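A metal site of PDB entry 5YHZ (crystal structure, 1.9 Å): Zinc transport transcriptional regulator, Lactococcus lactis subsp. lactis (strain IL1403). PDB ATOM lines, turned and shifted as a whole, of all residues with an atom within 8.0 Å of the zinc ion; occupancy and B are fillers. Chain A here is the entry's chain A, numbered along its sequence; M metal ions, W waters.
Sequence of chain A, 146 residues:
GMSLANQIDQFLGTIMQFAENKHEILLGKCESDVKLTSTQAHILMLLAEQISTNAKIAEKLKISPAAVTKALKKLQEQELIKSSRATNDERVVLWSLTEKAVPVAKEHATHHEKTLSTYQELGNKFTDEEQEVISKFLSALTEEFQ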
ATOM      1  N   LYS A  22      16.047 -24.758 -29.459  1.00  0.00           N
ATOM      2  CA  LYS A  22      16.606 -23.940 -28.379  1.00  0.00           C
ATOM      3  C   LYS A  22      16.200 -24.523 -27.018  1.00  0.00           C
ATOM      4  O   LYS A  22      15.280 -25.305 -26.939  1.00  0.00           O
ATOM      5  CB  LYS A  22      16.096 -22.488 -28.478  1.00  0.00           C
ATOM      6  CG  LYS A  22      16.140 -21.854 -29.897  1.00  0.00           C
ATOM      7  CD  LYS A  22      17.526 -21.913 -30.533  1.00  0.00           C
ATOM      8  CE  LYS A  22      17.683 -20.930 -31.720  1.00  0.00           C
ATOM      9  NZ  LYS A  22      17.952 -19.476 -31.345  1.00  0.00           N
ATOM     10  N   LEU A  26      12.774 -17.340 -25.334  1.00  0.00           N
ATOM     11  CA  LEU A  26      13.111 -15.933 -25.375  1.00  0.00           C
ATOM     12  C   LEU A  26      12.253 -15.271 -26.425  1.00  0.00           C
ATOM     13  O   LEU A  26      12.142 -15.788 -27.520  1.00  0.00           O
ATOM     14  CB  LEU A  26      14.606 -15.803 -25.775  1.00  0.00           C
ATOM     15  CG  LEU A  26      15.573 -16.155 -24.668  1.00  0.00           C
ATOM     16  CD1 LEU A  26      17.057 -16.283 -25.180  1.00  0.00           C
ATOM     17  CD2 LEU A  26      15.500 -15.089 -23.642  1.00  0.00           C
ATOM     18  N   LEU A  27      11.658 -14.124 -26.083  1.00  0.00           N
ATOM     19  CA  LEU A  27      10.889 -13.360 -27.038  1.00  0.00           C
ATOM     20  C   LEU A  27      11.829 -12.272 -27.643  1.00  0.00           C
ATOM     21  O   LEU A  27      12.929 -12.019 -27.134  1.00  0.00           O
ATOM     22  CB  LEU A  27       9.660 -12.708 -26.329  1.00  0.00           C
ATOM     23  CG  LEU A  27       8.662 -13.671 -25.658  1.00  0.00           C
ATOM     24  CD1 LEU A  27       7.559 -12.993 -24.769  1.00  0.00           C
ATOM     25  CD2 LEU A  27       8.019 -14.375 -26.804  1.00  0.00           C
ATOM     26  N   GLY A  28      11.364 -11.599 -28.674  1.00  0.00           N
ATOM     27  CA  GLY A  28      12.127 -10.504 -29.245  1.00  0.00           C
ATOM     28  C   GLY A  28      12.695 -10.974 -30.553  1.00  0.00           C
ATOM     29  O   GLY A  28      13.041 -12.122 -30.713  1.00  0.00           O
ATOM     30  N   LYS A  29      12.711 -10.075 -31.538  1.00  0.00           N
ATOM     31  CA  LYS A  29      13.282 -10.363 -32.832  1.00  0.00           C
ATOM     32  C   LYS A  29      14.728 -10.779 -32.587  1.00  0.00           C
ATOM     33  O   LYS A  29      15.439 -10.125 -31.819  1.00  0.00           O
ATOM     34  CB  LYS A  29      13.242  -9.079 -33.689  1.00  0.00           C
ATOM     35  CG  LYS A  29      13.464  -9.291 -35.170  1.00  0.00           C
ATOM     36  CD  LYS A  29      12.473 -10.256 -35.785  1.00  0.00           C
ATOM     37  CE  LYS A  29      12.412 -10.016 -37.303  1.00  0.00           C
ATOM     38  NZ  LYS A  29      13.798  -9.741 -37.843  1.00  0.00           N
ATOM     39  N   CYS A  30      15.157 -11.847 -33.237  1.00  0.00           N
ATOM     40  CA  CYS A  30      16.490 -12.398 -33.038  1.00  0.00           C
ATOM     41  C   CYS A  30      17.268 -12.364 -34.336  1.00  0.00           C
ATOM     42  O   CYS A  30      16.932 -13.090 -35.265  1.00  0.00           O
ATOM     43  CB  CYS A  30      16.387 -13.841 -32.557  1.00  0.00           C
ATOM     44  SG  CYS A  30      17.978 -14.604 -32.279  1.00  0.00           S
ATOM     45  N   GLU A  31      18.314 -11.528 -34.384  1.00  0.00           N
ATOM     46  CA  GLU A  31      19.139 -11.323 -35.585  1.00  0.00           C
ATOM     47  C   GLU A  31      20.397 -12.197 -35.624  1.00  0.00           C
ATOM     48  O   GLU A  31      20.777 -12.734 -36.676  1.00  0.00           O
ATOM     49  CB  GLU A  31      19.592  -9.876 -35.631  1.00  0.00           C
ATOM     50  CG  GLU A  31      19.663  -9.321 -37.030  1.00  0.00           C
ATOM     51  CD  GLU A  31      19.501  -7.826 -37.030  1.00  0.00           C
ATOM     52  OE1 GLU A  31      20.359  -7.140 -37.643  1.00  0.00           O
ATOM     53  OE2 GLU A  31      18.512  -7.321 -36.422  1.00  0.00           O
ATOM     54  N   SER A  32      21.040 -12.306 -34.471  1.00  0.00           N
ATOM     55  CA  SER A  32      22.289 -13.048 -34.348  1.00  0.00           C
ATOM     56  C   SER A  32      22.078 -14.457 -34.862  1.00  0.00           C
ATOM     57  O   SER A  32      20.969 -14.997 -34.846  1.00  0.00           O
ATOM     58  CB  SER A  32      22.771 -13.060 -32.882  1.00  0.00           C
ATOM     59  OG  SER A  32      23.847 -13.959 -32.672  1.00  0.00           O
ATOM     60  N   ASP A  33      23.153 -15.055 -35.361  1.00  0.00           N
ATOM     61  CA  ASP A  33      23.104 -16.413 -35.844  1.00  0.00           C
ATOM     62  C   ASP A  33      24.097 -17.226 -35.012  1.00  0.00           C
ATOM     63  O   ASP A  33      24.341 -18.395 -35.289  1.00  0.00           O
ATOM     64  CB  ASP A  33      23.439 -16.473 -37.344  1.00  0.00           C
ATOM     65  CG  ASP A  33      24.676 -15.653 -37.689  1.00  0.00           C
ATOM     66  OD1 ASP A  33      24.861 -14.539 -37.154  1.00  0.00           O
ATOM     67  OD2 ASP A  33      25.473 -16.138 -38.526  1.00  0.00           O
ATOM     68  N   VAL A  34      24.661 -16.580 -33.980  1.00  0.00           N
ATOM     69  CA  VAL A  34      25.693 -17.221 -33.152  1.00  0.00           C
ATOM     70  C   VAL A  34      25.094 -18.279 -32.233  1.00  0.00           C
ATOM     71  O   VAL A  34      24.599 -17.965 -31.165  1.00  0.00           O
ATOM     72  CB  VAL A  34      26.495 -16.180 -32.299  1.00  0.00           C
ATOM     73  CG1 VAL A  34      27.477 -16.898 -31.372  1.00  0.00           C
ATOM     74  CG2 VAL A  34      27.237 -15.158 -33.186  1.00  0.00           C
ATOM     75  N   PRO A 103      27.823  -7.393 -29.638  1.00  0.00           N
ATOM     76  CA  PRO A 103      26.414  -7.327 -30.046  1.00  0.00           C
ATOM     77  C   PRO A 103      25.658  -8.574 -29.678  1.00  0.00           C
ATOM     78  O   PRO A 103      24.432  -8.572 -29.639  1.00  0.00           O
ATOM     79  CB  PRO A 103      26.493  -7.184 -31.580  1.00  0.00           C
ATOM     80  CG  PRO A 103      27.837  -7.709 -31.945  1.00  0.00           C
ATOM     81  CD  PRO A 103      28.744  -7.381 -30.787  1.00  0.00           C
ATOM     82  N   VAL A 104      26.373  -9.643 -29.415  1.00  0.00           N
ATOM     83  CA  VAL A 104      25.742 -10.927 -29.182  1.00  0.00           C
ATOM     84  C   VAL A 104      25.238 -10.896 -27.772  1.00  0.00           C
ATOM     85  O   VAL A 104      24.073 -11.240 -27.541  1.00  0.00           O
ATOM     86  CB  VAL A 104      26.709 -12.090 -29.349  1.00  0.00           C
ATOM     87  CG1 VAL A 104      26.008 -13.445 -29.047  1.00  0.00           C
ATOM     88  CG2 VAL A 104      27.294 -12.094 -30.763  1.00  0.00           C
ATOM     89  N   LYS A 106      24.658  -8.124 -26.072  1.00  0.00           N
ATOM     90  CA  LYS A 106      23.705  -7.053 -25.891  1.00  0.00           C
ATOM     91  C   LYS A 106      22.359  -7.535 -26.442  1.00  0.00           C
ATOM     92  O   LYS A 106      21.323  -7.175 -25.896  1.00  0.00           O
ATOM     93  CB  LYS A 106      24.143  -5.778 -26.586  1.00  0.00           C
ATOM     94  CG  LYS A 106      23.001  -4.807 -26.810  1.00  0.00           C
ATOM     95  CD  LYS A 106      23.515  -3.420 -27.200  1.00  0.00           C
ATOM     96  CE  LYS A 106      22.374  -2.419 -27.373  1.00  0.00           C
ATOM     97  NZ  LYS A 106      22.878  -1.113 -27.932  1.00  0.00           N
ATOM     98  N   GLU A 107      22.397  -8.389 -27.472  1.00  0.00           N
ATOM     99  CA  GLU A 107      21.182  -8.933 -28.060  1.00  0.00           C
ATOM    100  C   GLU A 107      20.512  -9.917 -27.125  1.00  0.00           C
ATOM    101  O   GLU A 107      19.310  -9.910 -27.023  1.00  0.00           O
ATOM    102  CB  GLU A 107      21.400  -9.691 -29.359  1.00  0.00           C
ATOM    103  CG  GLU A 107      20.044 -10.192 -29.910  1.00  0.00           C
ATOM    104  CD  GLU A 107      20.121 -10.695 -31.329  1.00  0.00           C
ATOM    105  OE1 GLU A 107      21.171 -10.542 -31.982  1.00  0.00           O
ATOM    106  OE2 GLU A 107      19.107 -11.227 -31.826  1.00  0.00           O
ATOM    107  N   HIS A 108      21.295 -10.781 -26.493  1.00  0.00           N
ATOM    108  CA  HIS A 108      20.708 -11.802 -25.640  1.00  0.00           C
ATOM    109  C   HIS A 108      20.113 -11.134 -24.441  1.00  0.00           C
ATOM    110  O   HIS A 108      18.968 -11.418 -24.049  1.00  0.00           O
ATOM    111  CB  HIS A 108      21.730 -12.881 -25.294  1.00  0.00           C
ATOM    112  CG  HIS A 108      21.137 -14.101 -24.679  1.00  0.00           C
ATOM    113  ND1 HIS A 108      20.976 -15.274 -25.375  1.00  0.00           N
ATOM    114  CD2 HIS A 108      20.664 -14.347 -23.421  1.00  0.00           C
ATOM    115  CE1 HIS A 108      20.462 -16.200 -24.586  1.00  0.00           C
ATOM    116  NE2 HIS A 108      20.268 -15.657 -23.402  1.00  0.00           N
ATOM    117  N   ALA A 109      20.818 -10.149 -23.907  1.00  0.00           N
ATOM    118  CA  ALA A 109      20.335  -9.372 -22.787  1.00  0.00           C
ATOM    119  C   ALA A 109      19.040  -8.649 -23.136  1.00  0.00           C
ATOM    120  O   ALA A 109      18.208  -8.419 -22.283  1.00  0.00           O
ATOM    121  CB  ALA A 109      21.376  -8.372 -22.332  1.00  0.00           C
ATOM    122  N   THR A 110      18.932  -8.211 -24.375  1.00  0.00           N
ATOM    123  CA  THR A 110      17.749  -7.511 -24.831  1.00  0.00           C
ATOM    124  C   THR A 110      16.606  -8.514 -24.913  1.00  0.00           C
ATOM    125  O   THR A 110      15.469  -8.185 -24.638  1.00  0.00           O
ATOM    126  CB  THR A 110      18.017  -6.956 -26.224  1.00  0.00           C
ATOM    127  OG1 THR A 110      18.886  -5.844 -26.075  1.00  0.00           O
ATOM    128  CG2 THR A 110      16.729  -6.539 -26.914  1.00  0.00           C
ATOM    129  N   HIS A 111      16.909  -9.724 -25.335  1.00  0.00           N
ATOM    130  CA  HIS A 111      15.881 -10.748 -25.271  1.00  0.00           C
ATOM    131  C   HIS A 111      15.390 -10.943 -23.876  1.00  0.00           C
ATOM    132  O   HIS A 111      14.192 -11.071 -23.632  1.00  0.00           O
ATOM    133  CB  HIS A 111      16.420 -12.063 -25.758  1.00  0.00           C
ATOM    134  CG  HIS A 111      16.541 -12.123 -27.231  1.00  0.00           C
ATOM    135  ND1 HIS A 111      15.467 -11.984 -28.067  1.00  0.00           N
ATOM    136  CD2 HIS A 111      17.622 -12.313 -28.024  1.00  0.00           C
ATOM    137  CE1 HIS A 111      15.871 -12.088 -29.319  1.00  0.00           C
ATOM    138  NE2 HIS A 111      17.171 -12.286 -29.316  1.00  0.00           N
HETATM  139 ZN    ZN M   1      18.848 -13.084 -30.612  1.00  0.00          ZN
HETATM  140  O   HOH W   1      20.625 -13.719 -29.285  1.00  0.00           O
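A ring nitrogen (ND1) of His 111 is in hydrogen-bond range of the backbone carbonyl oxygen (O) of Leu 27 (2.7 Å). OE1 of Glu 107 sits at hydrogen-bond distance from N of Ser 32 (3.1 Å). The side-chain carboxylate (OE2) of Glu 107 sits close to the backbone NH (N) of Glu 31.
Within 4 Å of the zinc ion: Cys 30, Glu 107 and His 111. Along chain A the residues within 4 Å of the zinc ion span positions 30 to 111.
The zinc ion is bound by the side-chain carboxylate (OE2) of Glu 107, a ring nitrogen (NE2) of His 111, water W1 and the side-chain sulfur (SG) of Cys 30. The zinc ion has four donor atoms within binding distance.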
